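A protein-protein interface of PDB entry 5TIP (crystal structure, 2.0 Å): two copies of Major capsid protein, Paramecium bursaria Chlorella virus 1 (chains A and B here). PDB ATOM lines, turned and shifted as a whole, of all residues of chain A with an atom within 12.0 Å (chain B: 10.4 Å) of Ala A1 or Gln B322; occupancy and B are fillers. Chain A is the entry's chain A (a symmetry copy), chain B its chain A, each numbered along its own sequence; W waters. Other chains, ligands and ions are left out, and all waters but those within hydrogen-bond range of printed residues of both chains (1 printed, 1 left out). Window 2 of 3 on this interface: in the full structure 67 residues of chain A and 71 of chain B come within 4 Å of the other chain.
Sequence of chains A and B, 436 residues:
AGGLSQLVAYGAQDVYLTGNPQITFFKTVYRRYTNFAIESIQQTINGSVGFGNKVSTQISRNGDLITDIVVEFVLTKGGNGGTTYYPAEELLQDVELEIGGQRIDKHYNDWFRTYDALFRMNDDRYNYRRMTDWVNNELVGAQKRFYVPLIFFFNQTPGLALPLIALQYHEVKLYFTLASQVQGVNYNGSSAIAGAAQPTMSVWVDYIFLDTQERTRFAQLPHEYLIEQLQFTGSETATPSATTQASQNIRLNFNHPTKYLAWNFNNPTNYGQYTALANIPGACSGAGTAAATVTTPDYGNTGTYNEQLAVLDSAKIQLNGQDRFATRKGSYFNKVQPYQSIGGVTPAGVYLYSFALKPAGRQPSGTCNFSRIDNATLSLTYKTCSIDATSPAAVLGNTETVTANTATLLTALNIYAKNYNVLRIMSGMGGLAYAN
N of Gly A2 sits at hydrogen-bond distance from O of Asp B323 (2.9 Å). The guanidinium group (NE) of Arg B324 sits at hydrogen-bond distance from the side-chain amide oxygen (OE1) of Gln A6, 2.5 Å away.
The side-chain amino group (NZ) of Lys B316 lies within salt-bridge range of the side-chain carboxylate (OD2) of Asp B323. The backbone carbonyl oxygen (O) of Ile B317 sits at hydrogen-bond distance from the backbone NH (N) of Arg B324 (2.8 Å).
Among the printed residues, pairs that only touch across the chains: Gly A2 with Arg B324, Ala A1 with Gln B322, Gly A3 with Arg B324, Ser A5 with Leu B319, Ala A1 with Asp B323 and Ala A9 with Ile B373.
Of chain B, only Gln B322 and Asp B323 come within 4 Å of Ala A1. Gly A2 touches just these residues of chain B: Asp B323 (2.9 Å) and Arg B324 (3.3 Å). Printed residues of chain B within 4 Å of Ser A5: Leu B319 (3.8 Å). Of the printed residues of chain B, Gln A6 touches Arg B324. Of the printed residues of chain B, Ala A9 touches Ile B373 (3.995 Å). No residue of chain A comes within 4 Å of Gln B318. No residue of chain A comes within 4 Å of Asn B320. No residue of chain A comes within 4 Å of Gly B321. Gln B322 touches just one residue of chain A: Ala A1 (3.6 Å). Asp B323 touches just these residues of chain A: Ala A1 and Gly A2. The nearest residue of chain B that does not touch Ala A1 is Arg B324 (5.6 Å). The nearest residue of chain A that does not touch Gln B322 is Gly A2 (5.4 Å).
Of the 9 printed residues of chain A, 6 touch a printed residue of chain B. Of the 19 printed residues of chain B, 5 touch a printed residue of chain A. Among the printed residues, 8 pairs touch across the chains.
No position is printed for both chains.
Water W1 lies within hydrogen-bond range of OG of Ser A5 (2.5 Å) and O of Leu B319 (3.2 Å).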
ATOM      1  N   ALA A   1      -0.073  -2.786  20.381  1.00  0.00           N
ATOM      2  CA  ALA A   1       0.026  -4.000  21.184  1.00  0.00           C
ATOM      3  C   ALA A   1      -1.299  -4.747  21.195  1.00  0.00           C
ATOM      4  O   ALA A   1      -2.302  -4.263  20.673  1.00  0.00           O
ATOM      5  CB  ALA A   1       0.454  -3.666  22.603  1.00  0.00           C
ATOM      6  N   GLY A   2      -1.295  -5.933  21.794  1.00  0.00           N
ATOM      7  CA  GLY A   2      -2.508  -6.713  21.922  1.00  0.00           C
ATOM      8  C   GLY A   2      -2.928  -7.373  20.629  1.00  0.00           C
ATOM      9  O   GLY A   2      -2.084  -7.868  19.876  1.00  0.00           O
ATOM     10  N   GLY A   3      -4.236  -7.385  20.359  1.00  0.00           N
ATOM     11  CA  GLY A   3      -4.732  -8.050  19.165  1.00  0.00           C
ATOM     12  C   GLY A   3      -4.410  -7.318  17.878  1.00  0.00           C
ATOM     13  O   GLY A   3      -4.231  -7.949  16.833  1.00  0.00           O
ATOM     14  N   LEU A   4      -4.333  -5.987  17.929  1.00  0.00           N
ATOM     15  CA  LEU A   4      -4.049  -5.216  16.722  1.00  0.00           C
ATOM     16  C   LEU A   4      -2.665  -5.516  16.159  1.00  0.00           C
ATOM     17  O   LEU A   4      -2.485  -5.519  14.937  1.00  0.00           O
ATOM     18  CB  LEU A   4      -4.188  -3.724  17.017  1.00  0.00           C
ATOM     19  CG  LEU A   4      -4.588  -2.785  15.877  1.00  0.00           C
ATOM     20  CD1 LEU A   4      -3.395  -2.400  15.016  1.00  0.00           C
ATOM     21  CD2 LEU A   4      -5.675  -3.428  15.034  1.00  0.00           C
ATOM     22  N   SER A   5      -1.682  -5.786  17.021  1.00  0.00           N
ATOM     23  CA  SER A   5      -0.350  -6.119  16.523  1.00  0.00           C
ATOM     24  C   SER A   5      -0.301  -7.490  15.859  1.00  0.00           C
ATOM     25  O   SER A   5       0.588  -7.733  15.038  1.00  0.00           O
ATOM     26  CB  SER A   5       0.671  -6.063  17.655  1.00  0.00           C
ATOM     27  OG  SER A   5       1.977  -6.245  17.137  1.00  0.00           O
ATOM     28  N   GLN A   6      -1.236  -8.387  16.187  1.00  0.00           N
ATOM     29  CA  GLN A   6      -1.273  -9.693  15.538  1.00  0.00           C
ATOM     30  C   GLN A   6      -1.818  -9.593  14.119  1.00  0.00           C
ATOM     31  O   GLN A   6      -1.422 -10.379  13.249  1.00  0.00           O
ATOM     32  CB  GLN A   6      -2.097 -10.673  16.373  1.00  0.00           C
ATOM     33  CG  GLN A   6      -2.212 -12.066  15.770  1.00  0.00           C
ATOM     34  CD  GLN A   6      -2.978 -13.031  16.652  1.00  0.00           C
ATOM     35  OE1 GLN A   6      -2.723 -13.135  17.854  1.00  0.00           O
ATOM     36  NE2 GLN A   6      -3.930 -13.741  16.059  1.00  0.00           N
ATOM     37  N   LEU A   7      -2.721  -8.642  13.871  1.00  0.00           N
ATOM     38  CA  LEU A   7      -3.232  -8.443  12.519  1.00  0.00           C
ATOM     39  C   LEU A   7      -2.117  -8.031  11.566  1.00  0.00           C
ATOM     40  O   LEU A   7      -2.080  -8.473  10.412  1.00  0.00           O
ATOM     41  CB  LEU A   7      -4.344  -7.392  12.525  1.00  0.00           C
ATOM     42  CG  LEU A   7      -5.709  -7.856  13.028  1.00  0.00           C
ATOM     43  CD1 LEU A   7      -6.713  -6.714  12.975  1.00  0.00           C
ATOM     44  CD2 LEU A   7      -6.188  -9.046  12.216  1.00  0.00           C
ATOM     45  N   VAL A   8      -1.193  -7.185  12.033  1.00  0.00           N
ATOM     46  CA  VAL A   8      -0.094  -6.748  11.180  1.00  0.00           C
ATOM     47  C   VAL A   8       0.892  -7.878  10.918  1.00  0.00           C
ATOM     48  O   VAL A   8       1.585  -7.863   9.895  1.00  0.00           O
ATOM     49  CB  VAL A   8       0.614  -5.531  11.803  1.00  0.00           C
ATOM     50  CG1 VAL A   8       1.514  -4.852  10.777  1.00  0.00           C
ATOM     51  CG2 VAL A   8      -0.409  -4.550  12.350  1.00  0.00           C
ATOM     52  N   ALA A   9       0.966  -8.871  11.807  1.00  0.00           N
ATOM     53  CA  ALA A   9       1.806 -10.047  11.581  1.00  0.00           C
ATOM     54  C   ALA A   9       1.159 -10.872  10.474  1.00  0.00           C
ATOM     55  O   ALA A   9       0.525 -11.906  10.702  1.00  0.00           O
ATOM     56  CB  ALA A   9       1.971 -10.853  12.864  1.00  0.00           C
ATOM     57  N   LYS B 316       1.251 -14.839  30.560  1.00  0.00           N
ATOM     58  CA  LYS B 316       0.883 -13.968  29.454  1.00  0.00           C
ATOM     59  C   LYS B 316       1.898 -14.174  28.342  1.00  0.00           C
ATOM     60  O   LYS B 316       3.007 -14.660  28.571  1.00  0.00           O
ATOM     61  CB  LYS B 316       0.832 -12.494  29.869  1.00  0.00           C
ATOM     62  CG  LYS B 316       2.201 -11.870  30.112  1.00  0.00           C
ATOM     63  CD  LYS B 316       2.095 -10.385  30.423  1.00  0.00           C
ATOM     64  CE  LYS B 316       3.451  -9.797  30.788  1.00  0.00           C
ATOM     65  NZ  LYS B 316       3.346  -8.362  31.171  1.00  0.00           N
ATOM     66  N   ILE B 317       1.503 -13.797  27.132  1.00  0.00           N
ATOM     67  CA  ILE B 317       2.359 -13.895  25.958  1.00  0.00           C
ATOM     68  C   ILE B 317       2.734 -12.489  25.522  1.00  0.00           C
ATOM     69  O   ILE B 317       1.883 -11.593  25.481  1.00  0.00           O
ATOM     70  CB  ILE B 317       1.672 -14.662  24.812  1.00  0.00           C
ATOM     71  CG1 ILE B 317       1.315 -16.079  25.259  1.00  0.00           C
ATOM     72  CG2 ILE B 317       2.567 -14.703  23.583  1.00  0.00           C
ATOM     73  CD1 ILE B 317       0.544 -16.863  24.223  1.00  0.00           C
ATOM     74  N   GLN B 318       4.011 -12.292  25.208  1.00  0.00           N
ATOM     75  CA  GLN B 318       4.509 -11.015  24.724  1.00  0.00           C
ATOM     76  C   GLN B 318       4.904 -11.146  23.260  1.00  0.00           C
ATOM     77  O   GLN B 318       5.556 -12.120  22.865  1.00  0.00           O
ATOM     78  CB  GLN B 318       5.704 -10.533  25.551  1.00  0.00           C
ATOM     79  CG  GLN B 318       5.362 -10.188  26.995  1.00  0.00           C
ATOM     80  CD  GLN B 318       6.489  -9.464  27.709  1.00  0.00           C
ATOM     81  OE1 GLN B 318       7.257  -8.725  27.091  1.00  0.00           O
ATOM     82  NE2 GLN B 318       6.594  -9.672  29.018  1.00  0.00           N
ATOM     83  N   LEU B 319       4.510 -10.159  22.463  1.00  0.00           N
ATOM     84  CA  LEU B 319       4.768 -10.137  21.028  1.00  0.00           C
ATOM     85  C   LEU B 319       5.626  -8.915  20.740  1.00  0.00           C
ATOM     86  O   LEU B 319       5.132  -7.782  20.778  1.00  0.00           O
ATOM     87  CB  LEU B 319       3.456 -10.108  20.245  1.00  0.00           C
ATOM     88  CG  LEU B 319       3.443 -10.511  18.770  1.00  0.00           C
ATOM     89  CD1 LEU B 319       2.024 -10.860  18.359  1.00  0.00           C
ATOM     90  CD2 LEU B 319       3.989  -9.403  17.883  1.00  0.00           C
ATOM     91  N   ASN B 320       6.908  -9.149  20.457  1.00  0.00           N
ATOM     92  CA  ASN B 320       7.873  -8.078  20.209  1.00  0.00           C
ATOM     93  C   ASN B 320       7.938  -7.108  21.387  1.00  0.00           C
ATOM     94  O   ASN B 320       7.977  -5.889  21.213  1.00  0.00           O
ATOM     95  CB  ASN B 320       7.558  -7.341  18.905  1.00  0.00           C
ATOM     96  CG  ASN B 320       7.714  -8.229  17.686  1.00  0.00           C
ATOM     97  OD1 ASN B 320       8.589  -9.095  17.645  1.00  0.00           O
ATOM     98  ND2 ASN B 320       6.860  -8.025  16.688  1.00  0.00           N
ATOM     99  N   GLY B 321       7.947  -7.662  22.600  1.00  0.00           N
ATOM    100  CA  GLY B 321       8.076  -6.886  23.814  1.00  0.00           C
ATOM    101  C   GLY B 321       6.785  -6.334  24.380  1.00  0.00           C
ATOM    102  O   GLY B 321       6.771  -5.907  25.541  1.00  0.00           O
ATOM    103  N   GLN B 322       5.704  -6.332  23.608  1.00  0.00           N
ATOM    104  CA  GLN B 322       4.418  -5.817  24.054  1.00  0.00           C
ATOM    105  C   GLN B 322       3.464  -6.967  24.354  1.00  0.00           C
ATOM    106  O   GLN B 322       3.537  -8.033  23.737  1.00  0.00           O
ATOM    107  CB  GLN B 322       3.813  -4.874  23.012  1.00  0.00           C
ATOM    108  CG  GLN B 322       4.649  -3.626  22.783  1.00  0.00           C
ATOM    109  CD  GLN B 322       4.765  -2.770  24.031  1.00  0.00           C
ATOM    110  OE1 GLN B 322       3.787  -2.560  24.748  1.00  0.00           O
ATOM    111  NE2 GLN B 322       5.970  -2.285  24.304  1.00  0.00           N
ATOM    112  N   ASP B 323       2.570  -6.739  25.313  1.00  0.00           N
ATOM    113  CA  ASP B 323       1.637  -7.775  25.745  1.00  0.00           C
ATOM    114  C   ASP B 323       0.653  -8.117  24.633  1.00  0.00           C
ATOM    115  O   ASP B 323      -0.060  -7.243  24.130  1.00  0.00           O
ATOM    116  CB  ASP B 323       0.879  -7.319  26.989  1.00  0.00           C
ATOM    117  CG  ASP B 323       1.775  -7.171  28.200  1.00  0.00           C
ATOM    118  OD1 ASP B 323       3.006  -7.322  28.053  1.00  0.00           O
ATOM    119  OD2 ASP B 323       1.246  -6.910  29.301  1.00  0.00           O
ATOM    120  N   ARG B 324       0.621  -9.394  24.244  1.00  0.00           N
ATOM    121  CA  ARG B 324      -0.425  -9.866  23.344  1.00  0.00           C
ATOM    122  C   ARG B 324      -1.774  -9.895  24.049  1.00  0.00           C
ATOM    123  O   ARG B 324      -2.813  -9.677  23.415  1.00  0.00           O
ATOM    124  CB  ARG B 324      -0.059 -11.249  22.801  1.00  0.00           C
ATOM    125  CG  ARG B 324      -1.146 -11.930  21.984  1.00  0.00           C
ATOM    126  CD  ARG B 324      -1.540 -11.110  20.771  1.00  0.00           C
ATOM    127  NE  ARG B 324      -2.562 -11.788  19.981  1.00  0.00           N
ATOM    128  CZ  ARG B 324      -3.859 -11.771  20.270  1.00  0.00           C
ATOM    129  NH1 ARG B 324      -4.296 -11.111  21.334  1.00  0.00           N
ATOM    130  NH2 ARG B 324      -4.720 -12.419  19.497  1.00  0.00           N
ATOM    131  N   PHE B 325      -1.772 -10.151  25.356  1.00  0.00           N
ATOM    132  CA  PHE B 325      -2.968 -10.053  26.177  1.00  0.00           C
ATOM    133  C   PHE B 325      -2.538  -9.855  27.622  1.00  0.00           C
ATOM    134  O   PHE B 325      -1.384 -10.104  27.985  1.00  0.00           O
ATOM    135  CB  PHE B 325      -3.869 -11.287  26.031  1.00  0.00           C
ATOM    136  CG  PHE B 325      -3.152 -12.596  26.212  1.00  0.00           C
ATOM    137  CD1 PHE B 325      -3.022 -13.163  27.469  1.00  0.00           C
ATOM    138  CD2 PHE B 325      -2.619 -13.264  25.123  1.00  0.00           C
ATOM    139  CE1 PHE B 325      -2.366 -14.369  27.638  1.00  0.00           C
ATOM    140  CE2 PHE B 325      -1.961 -14.469  25.285  1.00  0.00           C
ATOM    141  CZ  PHE B 325      -1.836 -15.022  26.543  1.00  0.00           C
ATOM    142  N   ALA B 326      -3.480  -9.393  28.439  1.00  0.00           N
ATOM    143  CA  ALA B 326      -3.204  -9.155  29.849  1.00  0.00           C
ATOM    144  C   ALA B 326      -3.007 -10.470  30.592  1.00  0.00           C
ATOM    145  O   ALA B 326      -3.510 -11.522  30.188  1.00  0.00           O
ATOM    146  CB  ALA B 326      -4.337  -8.354  30.490  1.00  0.00           C
ATOM    147  N   THR B 327      -2.263 -10.398  31.692  1.00  0.00           N
ATOM    148  CA  THR B 327      -1.925 -11.592  32.454  1.00  0.00           C
ATOM    149  C   THR B 327      -3.174 -12.235  33.042  1.00  0.00           C
ATOM    150  O   THR B 327      -4.011 -11.560  33.650  1.00  0.00           O
ATOM    151  CB  THR B 327      -0.948 -11.238  33.575  1.00  0.00           C
ATOM    152  OG1 THR B 327       0.217 -10.615  33.019  1.00  0.00           O
ATOM    153  CG2 THR B 327      -0.532 -12.483  34.331  1.00  0.00           C
ATOM    154  N   ILE B 373       6.819 -12.804  13.305  1.00  0.00           N
ATOM    155  CA  ILE B 373       7.028 -12.261  14.641  1.00  0.00           C
ATOM    156  C   ILE B 373       8.476 -12.519  15.023  1.00  0.00           C
ATOM    157  O   ILE B 373       8.914 -13.675  15.085  1.00  0.00           O
ATOM    158  CB  ILE B 373       6.067 -12.880  15.666  1.00  0.00           C
ATOM    159  CG1 ILE B 373       4.620 -12.726  15.196  1.00  0.00           C
ATOM    160  CG2 ILE B 373       6.269 -12.244  17.031  1.00  0.00           C
ATOM    161  CD1 ILE B 373       3.624 -13.441  16.070  1.00  0.00           C
ATOM    162  N   ASP B 374       9.220 -11.440  15.278  1.00  0.00           N
ATOM    163  CA  ASP B 374      10.627 -11.587  15.633  1.00  0.00           C
ATOM    164  C   ASP B 374      10.788 -12.131  17.047  1.00  0.00           C
ATOM    165  O   ASP B 374      11.624 -13.010  17.285  1.00  0.00           O
ATOM    166  CB  ASP B 374      11.344 -10.244  15.491  1.00  0.00           C
ATOM    167  CG  ASP B 374      11.553  -9.845  14.044  1.00  0.00           C
ATOM    168  OD1 ASP B 374      11.593 -10.746  13.179  1.00  0.00           O
ATOM    169  OD2 ASP B 374      11.680  -8.634  13.770  1.00  0.00           O
ATOM    170  N   ASN B 375       9.999 -11.629  17.994  1.00  0.00           N
ATOM    171  CA  ASN B 375      10.116 -12.023  19.393  1.00  0.00           C
ATOM    172  C   ASN B 375       8.736 -12.380  19.925  1.00  0.00           C
ATOM    173  O   ASN B 375       7.878 -11.505  20.080  1.00  0.00           O
ATOM    174  CB  ASN B 375      10.752 -10.909  20.229  1.00  0.00           C
ATOM    175  CG  ASN B 375      11.030 -11.335  21.665  1.00  0.00           C
ATOM    176  OD1 ASN B 375      10.139 -11.804  22.375  1.00  0.00           O
ATOM    177  ND2 ASN B 375      12.275 -11.175  22.095  1.00  0.00           N
ATOM    178  N   ALA B 376       8.527 -13.662  20.206  1.00  0.00           N
ATOM    179  CA  ALA B 376       7.343 -14.143  20.901  1.00  0.00           C
ATOM    180  C   ALA B 376       7.805 -14.818  22.182  1.00  0.00           C
ATOM    181  O   ALA B 376       8.650 -15.718  22.141  1.00  0.00           O
ATOM    182  CB  ALA B 376       6.537 -15.116  20.039  1.00  0.00           C
ATOM    183  N   THR B 377       7.249 -14.393  23.311  1.00  0.00           N
ATOM    184  CA  THR B 377       7.720 -14.837  24.613  1.00  0.00           C
ATOM    185  C   THR B 377       6.543 -15.231  25.490  1.00  0.00           C
ATOM    186  O   THR B 377       5.518 -14.543  25.518  1.00  0.00           O
ATOM    187  CB  THR B 377       8.541 -13.735  25.300  1.00  0.00           C
ATOM    188  OG1 THR B 377       9.649 -13.375  24.465  1.00  0.00           O
ATOM    189  CG2 THR B 377       9.062 -14.209  26.645  1.00  0.00           C
ATOM    190  N   LEU B 378       6.697 -16.342  26.203  1.00  0.00           N
ATOM    191  CA  LEU B 378       5.722 -16.792  27.188  1.00  0.00           C
ATOM    192  C   LEU B 378       6.232 -16.415  28.574  1.00  0.00           C
ATOM    193  O   LEU B 378       7.183 -17.021  29.079  1.00  0.00           O
ATOM    194  CB  LEU B 378       5.494 -18.298  27.077  1.00  0.00           C
ATOM    195  CG  LEU B 378       4.532 -18.910  28.096  1.00  0.00           C
ATOM    196  CD1 LEU B 378       3.122 -18.370  27.910  1.00  0.00           C
ATOM    197  CD2 LEU B 378       4.548 -20.429  28.009  1.00  0.00           C
ATOM    198  N   SER B 379       5.610 -15.409  29.182  1.00  0.00           N
ATOM    199  CA  SER B 379       5.999 -14.944  30.506  1.00  0.00           C
ATOM    200  C   SER B 379       5.229 -15.739  31.554  1.00  0.00           C
ATOM    201  O   SER B 379       3.994 -15.715  31.572  1.00  0.00           O
ATOM    202  CB  SER B 379       5.734 -13.447  30.655  1.00  0.00           C
ATOM    203  OG  SER B 379       6.172 -12.972  31.916  1.00  0.00           O
HETATM  204  O   HOH W   1       3.933  -5.769  18.645  1.00  0.00           O
